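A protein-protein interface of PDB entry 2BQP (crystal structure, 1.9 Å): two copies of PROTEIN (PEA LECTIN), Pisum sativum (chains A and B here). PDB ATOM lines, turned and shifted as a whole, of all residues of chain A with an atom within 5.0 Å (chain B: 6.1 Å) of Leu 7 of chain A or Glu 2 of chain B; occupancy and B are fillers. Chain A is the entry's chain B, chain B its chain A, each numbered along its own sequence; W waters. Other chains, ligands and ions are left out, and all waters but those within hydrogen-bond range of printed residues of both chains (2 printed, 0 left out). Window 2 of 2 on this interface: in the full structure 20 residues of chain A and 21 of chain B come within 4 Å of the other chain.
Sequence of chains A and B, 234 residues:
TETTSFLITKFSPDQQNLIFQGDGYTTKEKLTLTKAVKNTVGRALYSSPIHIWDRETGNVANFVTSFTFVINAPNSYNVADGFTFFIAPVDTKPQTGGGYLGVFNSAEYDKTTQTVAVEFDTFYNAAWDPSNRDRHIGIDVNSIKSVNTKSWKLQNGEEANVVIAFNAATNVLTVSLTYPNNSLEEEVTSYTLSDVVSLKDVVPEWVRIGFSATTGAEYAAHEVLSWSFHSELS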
ATOM      1  N   SER A   5     -16.958  28.663   4.220  1.00  0.00           N
ATOM      2  CA  SER A   5     -17.987  27.703   4.581  1.00  0.00           C
ATOM      3  C   SER A   5     -18.018  26.588   3.575  1.00  0.00           C
ATOM      4  O   SER A   5     -17.595  26.758   2.429  1.00  0.00           O
ATOM      5  CB  SER A   5     -19.383  28.333   4.564  1.00  0.00           C
ATOM      6  OG  SER A   5     -19.496  29.395   5.495  1.00  0.00           O
ATOM      7  N   PHE A   6     -18.537  25.447   4.001  1.00  0.00           N
ATOM      8  CA  PHE A   6     -18.733  24.324   3.116  1.00  0.00           C
ATOM      9  C   PHE A   6     -19.646  23.339   3.807  1.00  0.00           C
ATOM     10  O   PHE A   6     -19.736  23.341   5.034  1.00  0.00           O
ATOM     11  CB  PHE A   6     -17.409  23.714   2.620  1.00  0.00           C
ATOM     12  CG  PHE A   6     -16.683  22.882   3.636  1.00  0.00           C
ATOM     13  CD1 PHE A   6     -17.046  21.552   3.851  1.00  0.00           C
ATOM     14  CD2 PHE A   6     -15.618  23.422   4.358  1.00  0.00           C
ATOM     15  CE1 PHE A   6     -16.351  20.763   4.780  1.00  0.00           C
ATOM     16  CE2 PHE A   6     -14.918  22.641   5.285  1.00  0.00           C
ATOM     17  CZ  PHE A   6     -15.287  21.311   5.493  1.00  0.00           C
ATOM     18  N   LEU A   7     -20.408  22.590   3.024  1.00  0.00           N
ATOM     19  CA  LEU A   7     -21.338  21.592   3.532  1.00  0.00           C
ATOM     20  C   LEU A   7     -21.343  20.429   2.558  1.00  0.00           C
ATOM     21  O   LEU A   7     -21.463  20.637   1.345  1.00  0.00           O
ATOM     22  CB  LEU A   7     -22.771  22.157   3.611  1.00  0.00           C
ATOM     23  CG  LEU A   7     -23.899  21.108   3.696  1.00  0.00           C
ATOM     24  CD1 LEU A   7     -23.993  20.592   5.098  1.00  0.00           C
ATOM     25  CD2 LEU A   7     -25.263  21.632   3.244  1.00  0.00           C
ATOM     26  N   ILE A   8     -21.195  19.212   3.063  1.00  0.00           N
ATOM     27  CA  ILE A   8     -21.248  18.034   2.200  1.00  0.00           C
ATOM     28  C   ILE A   8     -22.171  17.087   2.930  1.00  0.00           C
ATOM     29  O   ILE A   8     -21.890  16.716   4.066  1.00  0.00           O
ATOM     30  CB  ILE A   8     -19.847  17.348   2.012  1.00  0.00           C
ATOM     31  CG1 ILE A   8     -18.832  18.323   1.425  1.00  0.00           C
ATOM     32  CG2 ILE A   8     -19.975  16.111   1.114  1.00  0.00           C
ATOM     33  CD1 ILE A   8     -17.393  18.018   1.827  1.00  0.00           C
ATOM     34  N   THR A   9     -23.311  16.761   2.336  1.00  0.00           N
ATOM     35  CA  THR A   9     -24.245  15.847   2.995  1.00  0.00           C
ATOM     36  C   THR A   9     -24.193  14.457   2.366  1.00  0.00           C
ATOM     37  O   THR A   9     -24.897  13.534   2.792  1.00  0.00           O
ATOM     38  CB  THR A   9     -25.695  16.368   2.942  1.00  0.00           C
ATOM     39  OG1 THR A   9     -26.245  16.143   1.634  1.00  0.00           O
ATOM     40  CG2 THR A   9     -25.731  17.841   3.245  1.00  0.00           C
ATOM     41  N   LYS A  10     -23.383  14.318   1.331  1.00  0.00           N
ATOM     42  CA  LYS A  10     -23.242  13.051   0.644  1.00  0.00           C
ATOM     43  C   LYS A  10     -21.878  13.126  -0.016  1.00  0.00           C
ATOM     44  O   LYS A  10     -21.548  14.134  -0.656  1.00  0.00           O
ATOM     45  CB  LYS A  10     -24.349  12.900  -0.409  1.00  0.00           C
ATOM     46  CG  LYS A  10     -24.319  11.575  -1.168  1.00  0.00           C
ATOM     47  CD  LYS A  10     -25.391  11.480  -2.250  1.00  0.00           C
ATOM     48  CE  LYS A  10     -26.783  11.321  -1.638  1.00  0.00           C
ATOM     49  NZ  LYS A  10     -27.859  11.187  -2.680  1.00  0.00           N
ATOM     50  N   SER A  12     -18.948  11.781  -2.661  1.00  0.00           N
ATOM     51  CA  SER A  12     -18.869  11.132  -3.960  1.00  0.00           C
ATOM     52  C   SER A  12     -17.580  10.328  -4.127  1.00  0.00           C
ATOM     53  O   SER A  12     -16.579  10.608  -3.464  1.00  0.00           O
ATOM     54  CB  SER A  12     -18.997  12.181  -5.083  1.00  0.00           C
ATOM     55  OG  SER A  12     -18.229  13.340  -4.831  1.00  0.00           O
ATOM     56  N   GLN A  15     -14.240  12.805  -4.484  1.00  0.00           N
ATOM     57  CA  GLN A  15     -14.551  14.011  -3.752  1.00  0.00           C
ATOM     58  C   GLN A  15     -13.327  14.884  -3.821  1.00  0.00           C
ATOM     59  O   GLN A  15     -12.515  14.911  -2.907  1.00  0.00           O
ATOM     60  CB  GLN A  15     -14.946  13.643  -2.330  1.00  0.00           C
ATOM     61  CG  GLN A  15     -15.635  14.719  -1.564  1.00  0.00           C
ATOM     62  CD  GLN A  15     -16.938  15.120  -2.165  1.00  0.00           C
ATOM     63  OE1 GLN A  15     -17.829  14.287  -2.377  1.00  0.00           O
ATOM     64  NE2 GLN A  15     -17.071  16.406  -2.463  1.00  0.00           N
ATOM     65  N   ASN A  17     -12.702  18.027  -3.405  1.00  0.00           N
ATOM     66  CA  ASN A  17     -12.405  19.132  -2.515  1.00  0.00           C
ATOM     67  C   ASN A  17     -11.825  18.677  -1.164  1.00  0.00           C
ATOM     68  O   ASN A  17     -11.549  19.501  -0.272  1.00  0.00           O
ATOM     69  CB  ASN A  17     -13.602  20.078  -2.359  1.00  0.00           C
ATOM     70  CG  ASN A  17     -14.856  19.374  -1.969  1.00  0.00           C
ATOM     71  OD1 ASN A  17     -14.945  18.145  -2.008  1.00  0.00           O
ATOM     72  ND2 ASN A  17     -15.852  20.145  -1.590  1.00  0.00           N
ATOM     73  N   TRP A 227     -20.701  16.584   6.717  1.00  0.00           N
ATOM     74  CA  TRP A 227     -19.782  17.545   7.323  1.00  0.00           C
ATOM     75  C   TRP A 227     -20.038  18.962   6.836  1.00  0.00           C
ATOM     76  O   TRP A 227     -20.186  19.198   5.633  1.00  0.00           O
ATOM     77  CB  TRP A 227     -18.353  17.141   6.918  1.00  0.00           C
ATOM     78  CG  TRP A 227     -17.209  17.917   7.541  1.00  0.00           C
ATOM     79  CD1 TRP A 227     -17.241  18.646   8.702  1.00  0.00           C
ATOM     80  CD2 TRP A 227     -15.847  17.982   7.071  1.00  0.00           C
ATOM     81  NE1 TRP A 227     -15.989  19.156   8.984  1.00  0.00           N
ATOM     82  CE2 TRP A 227     -15.114  18.764   8.004  1.00  0.00           C
ATOM     83  CE3 TRP A 227     -15.174  17.453   5.960  1.00  0.00           C
ATOM     84  CZ2 TRP A 227     -13.744  19.027   7.860  1.00  0.00           C
ATOM     85  CZ3 TRP A 227     -13.814  17.716   5.822  1.00  0.00           C
ATOM     86  CH2 TRP A 227     -13.112  18.498   6.771  1.00  0.00           C
ATOM     87  N   SER A 228     -20.053  19.910   7.755  1.00  0.00           N
ATOM     88  CA  SER A 228     -20.227  21.292   7.394  1.00  0.00           C
ATOM     89  C   SER A 228     -19.260  22.062   8.252  1.00  0.00           C
ATOM     90  O   SER A 228     -18.913  21.635   9.340  1.00  0.00           O
ATOM     91  CB  SER A 228     -21.666  21.759   7.628  1.00  0.00           C
ATOM     92  OG  SER A 228     -21.947  21.934   8.998  1.00  0.00           O
ATOM     93  N   THR B   1     -26.660  17.109  -1.149  1.00  0.00           N
ATOM     94  CA  THR B   1     -26.387  18.565  -1.222  1.00  0.00           C
ATOM     95  C   THR B   1     -24.934  18.871  -0.905  1.00  0.00           C
ATOM     96  O   THR B   1     -24.349  18.264  -0.021  1.00  0.00           O
ATOM     97  CB  THR B   1     -27.287  19.334  -0.257  1.00  0.00           C
ATOM     98  OG1 THR B   1     -28.657  19.019  -0.546  1.00  0.00           O
ATOM     99  CG2 THR B   1     -27.055  20.851  -0.385  1.00  0.00           C
ATOM    100  N   GLU B   2     -24.355  19.801  -1.649  1.00  0.00           N
ATOM    101  CA  GLU B   2     -22.986  20.186  -1.455  1.00  0.00           C
ATOM    102  C   GLU B   2     -22.903  21.678  -1.725  1.00  0.00           C
ATOM    103  O   GLU B   2     -23.450  22.153  -2.715  1.00  0.00           O
ATOM    104  CB  GLU B   2     -22.121  19.384  -2.428  1.00  0.00           C
ATOM    105  CG  GLU B   2     -20.640  19.657  -2.333  1.00  0.00           C
ATOM    106  CD  GLU B   2     -19.782  18.637  -3.070  1.00  0.00           C
ATOM    107  OE1 GLU B   2     -20.295  17.574  -3.509  1.00  0.00           O
ATOM    108  OE2 GLU B   2     -18.574  18.917  -3.190  1.00  0.00           O
ATOM    109  N   THR B   3     -22.294  22.438  -0.820  1.00  0.00           N
ATOM    110  CA  THR B   3     -22.167  23.876  -1.015  1.00  0.00           C
ATOM    111  C   THR B   3     -20.759  24.354  -0.680  1.00  0.00           C
ATOM    112  O   THR B   3     -20.046  23.720   0.111  1.00  0.00           O
ATOM    113  CB  THR B   3     -23.207  24.709  -0.190  1.00  0.00           C
ATOM    114  OG1 THR B   3     -22.644  25.086   1.068  1.00  0.00           O
ATOM    115  CG2 THR B   3     -24.488  23.906   0.053  1.00  0.00           C
ATOM    116  N   THR B   4     -20.372  25.474  -1.283  1.00  0.00           N
ATOM    117  CA  THR B   4     -19.059  26.060  -1.073  1.00  0.00           C
ATOM    118  C   THR B   4     -19.242  27.561  -1.020  1.00  0.00           C
ATOM    119  O   THR B   4     -19.957  28.113  -1.870  1.00  0.00           O
ATOM    120  CB  THR B   4     -18.144  25.742  -2.255  1.00  0.00           C
ATOM    121  OG1 THR B   4     -18.090  24.325  -2.432  1.00  0.00           O
ATOM    122  CG2 THR B   4     -16.745  26.287  -2.026  1.00  0.00           C
ATOM    123  N   ILE B  50     -14.419  23.182  -7.038  1.00  0.00           N
ATOM    124  CA  ILE B  50     -15.848  23.341  -6.773  1.00  0.00           C
ATOM    125  C   ILE B  50     -16.602  22.244  -7.498  1.00  0.00           C
ATOM    126  O   ILE B  50     -16.237  21.857  -8.606  1.00  0.00           O
ATOM    127  CB  ILE B  50     -16.406  24.704  -7.334  1.00  0.00           C
ATOM    128  CG1 ILE B  50     -15.521  25.888  -6.941  1.00  0.00           C
ATOM    129  CG2 ILE B  50     -17.858  24.898  -6.925  1.00  0.00           C
ATOM    130  CD1 ILE B  50     -15.418  26.172  -5.468  1.00  0.00           C
ATOM    131  N   HIS B  51     -17.658  21.735  -6.885  1.00  0.00           N
ATOM    132  CA  HIS B  51     -18.453  20.722  -7.538  1.00  0.00           C
ATOM    133  C   HIS B  51     -19.561  21.457  -8.303  1.00  0.00           C
ATOM    134  O   HIS B  51     -20.615  21.789  -7.733  1.00  0.00           O
ATOM    135  CB  HIS B  51     -19.046  19.754  -6.520  1.00  0.00           C
ATOM    136  CG  HIS B  51     -19.331  18.412  -7.104  1.00  0.00           C
ATOM    137  ND1 HIS B  51     -19.725  17.330  -6.344  1.00  0.00           N
ATOM    138  CD2 HIS B  51     -19.288  17.980  -8.387  1.00  0.00           C
ATOM    139  CE1 HIS B  51     -19.920  16.290  -7.142  1.00  0.00           C
ATOM    140  NE2 HIS B  51     -19.661  16.663  -8.384  1.00  0.00           N
ATOM    141  N   TRP B 206     -15.832  19.091 -11.789  1.00  0.00           N
ATOM    142  CA  TRP B 206     -15.064  19.698 -10.718  1.00  0.00           C
ATOM    143  C   TRP B 206     -14.265  20.780 -11.422  1.00  0.00           C
ATOM    144  O   TRP B 206     -13.600  20.518 -12.422  1.00  0.00           O
ATOM    145  CB  TRP B 206     -14.150  18.664 -10.062  1.00  0.00           C
ATOM    146  CG  TRP B 206     -14.877  17.795  -9.062  1.00  0.00           C
ATOM    147  CD1 TRP B 206     -15.350  16.521  -9.248  1.00  0.00           C
ATOM    148  CD2 TRP B 206     -15.207  18.149  -7.719  1.00  0.00           C
ATOM    149  NE1 TRP B 206     -15.951  16.062  -8.094  1.00  0.00           N
ATOM    150  CE2 TRP B 206     -15.878  17.045  -7.143  1.00  0.00           C
ATOM    151  CE3 TRP B 206     -14.985  19.293  -6.939  1.00  0.00           C
ATOM    152  CZ2 TRP B 206     -16.332  17.048  -5.817  1.00  0.00           C
ATOM    153  CZ3 TRP B 206     -15.432  19.298  -5.616  1.00  0.00           C
ATOM    154  CH2 TRP B 206     -16.097  18.176  -5.071  1.00  0.00           C
ATOM    155  N   SER B 231     -21.814  28.717  -3.967  1.00  0.00           N
ATOM    156  CA  SER B 231     -22.391  27.778  -4.896  1.00  0.00           C
ATOM    157  C   SER B 231     -23.209  26.735  -4.134  1.00  0.00           C
ATOM    158  O   SER B 231     -22.971  26.471  -2.937  1.00  0.00           O
ATOM    159  CB  SER B 231     -21.314  27.134  -5.787  1.00  0.00           C
ATOM    160  OG  SER B 231     -20.441  26.291  -5.057  1.00  0.00           O
ATOM    161  N   GLU B 232     -24.196  26.172  -4.813  1.00  0.00           N
ATOM    162  CA  GLU B 232     -25.045  25.178  -4.208  1.00  0.00           C
ATOM    163  C   GLU B 232     -25.440  24.127  -5.235  1.00  0.00           C
ATOM    164  O   GLU B 232     -26.061  24.444  -6.260  1.00  0.00           O
ATOM    165  CB  GLU B 232     -26.277  25.879  -3.655  1.00  0.00           C
ATOM    166  CG  GLU B 232     -27.069  25.098  -2.628  1.00  0.00           C
ATOM    167  CD  GLU B 232     -28.155  25.957  -1.999  1.00  0.00           C
ATOM    168  OE1 GLU B 232     -27.817  27.048  -1.472  1.00  0.00           O
ATOM    169  OE2 GLU B 232     -29.341  25.552  -2.041  1.00  0.00           O
ATOM    170  N   LEU B 233     -25.031  22.887  -4.989  1.00  0.00           N
ATOM    171  CA  LEU B 233     -25.342  21.762  -5.864  1.00  0.00           C
ATOM    172  C   LEU B 233     -26.233  20.839  -5.056  1.00  0.00           C
ATOM    173  O   LEU B 233     -25.810  20.341  -4.009  1.00  0.00           O
ATOM    174  CB  LEU B 233     -24.053  21.031  -6.264  1.00  0.00           C
ATOM    175  CG  LEU B 233     -24.180  19.694  -7.008  1.00  0.00           C
ATOM    176  CD1 LEU B 233     -24.843  19.869  -8.355  1.00  0.00           C
ATOM    177  CD2 LEU B 233     -22.799  19.102  -7.196  1.00  0.00           C
ATOM    178  N   SER B 234     -27.466  20.628  -5.499  1.00  0.00           N
ATOM    179  CA  SER B 234     -28.382  19.767  -4.750  1.00  0.00           C
ATOM    180  C   SER B 234     -28.279  18.289  -5.119  1.00  0.00           C
ATOM    181  O   SER B 234     -28.700  17.459  -4.270  1.00  0.00           O
ATOM    182  CB  SER B 234     -29.829  20.239  -4.903  1.00  0.00           C
ATOM    183  OG  SER B 234     -30.291  20.078  -6.237  1.00  0.00           O
ATOM    184  OXT SER B 234     -27.770  17.983  -6.228  1.00  0.00           O
HETATM  185  O   HOH W   1     -21.249  26.954   2.421  1.00  0.00           O
HETATM  186  O   HOH W   2     -15.136  22.902  -1.981  1.00  0.00           O
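Among the printed residues, merely in contact across the chains: Leu 7 of chain A with Glu 2 of chain B, Asn 17 of chain A with Trp 206 of chain B, Gln 15 of chain A with Trp 206 of chain B, Phe 6 of chain A with Thr 3 of chain B, Ile 8 of chain A with Thr 1 of chain B, Ser 5 of chain A with Thr 4 of chain B and Leu 7 of chain A with Thr 1 of chain B.
The side-chain carboxylate (OE1) of Glu 2 of chain B lies within hydrogen-bond range of a ring nitrogen (ND1) of His 51 of chain B (2.9 Å). The backbone NH of Glu 2 of chain B lies within hydrogen-bond range of the backbone carbonyl oxygen of Leu 233 of chain B, at 2.8 Å. The backbone carbonyl oxygen (O) of Thr 4 of chain B lies within hydrogen-bond range of the backbone NH (N) of Ser 231 of chain B, at 2.9 Å. The backbone NH (N) of Ile 8 of chain A sits at hydrogen-bond distance from the backbone carbonyl oxygen (O) of Trp 227 of chain A. The side-chain hydroxyl of Ser 12 of chain A is in hydrogen-bond range of the side-chain amide oxygen of Gln 15 of chain A, 2.7 Å away. NE2 of Gln 15 of chain A is in hydrogen-bond range of OD1 of Asn 17 of chain A, at 2.8 Å.
Printed residues of chain B within 4 Å of Phe 6 of chain A: Thr 3 (3.3 Å). Of chain B, only Thr 1 (3.98 Å), Glu 2 (3.2 Å) and Thr 3 (2.9 Å) come within 4 Å of Leu 7 of chain A. Of the printed residues of chain B, Asn 17 of chain A touches Glu 2 (3.4 Å) and Trp 206 (3.3 Å). Glu 2 of chain B touches just these residues of chain A: Leu 7, Gln 15 and Asn 17. Of the printed residues of chain A, Thr 4 of chain B touches Ser 5 (3.9 Å). Glu 232 of chain B touches none of the printed residues of chain A.
Water W1 lies within hydrogen-bond range of OG1 of Thr 3 of chain B (2.7 Å) and N of Phe 6 of chain A (3.5 Å). Water W2 bridges the side-chain amide nitrogen (ND2) of Asn 17 of chain A and the side-chain hydroxyl (OG1) of Thr 4 of chain B.
The backbone NH (N) of Thr 1 of chain B is in hydrogen-bond range of the side-chain hydroxyl (OG1) of Thr 9 of chain A, at 3.0 Å. The side-chain carboxylate (OE2) of Glu 2 of chain B is in hydrogen-bond range of the side-chain amide nitrogen (NE2) of Gln 15 of chain A (3.0 Å). ND2 of Asn 17 of chain A sits at hydrogen-bond distance from OE2 of Glu 2 of chain B (3.4 Å). N of Thr 3 of chain B sits at hydrogen-bond distance from O of Leu 7 of chain A (2.9 Å).
Of the 11 printed residues of chain B, 5 touch a printed residue of chain A. Hydrophobic or aromatic side chains of chain B that line the printed part of chain A: Trp 206. Printed residues of chain A that touch a printed residue of chain B: Ser 5, Phe 6, Leu 7, Ile 8, Thr 9, Gln 15 and Asn 17. Among the printed residues, 11 pairs touch across the chains. Among the printed residues, no Asp or Glu carboxylate lies within 4 Å of a Lys or Arg side-chain nitrogen of the other chain.
No position is printed for both chains.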
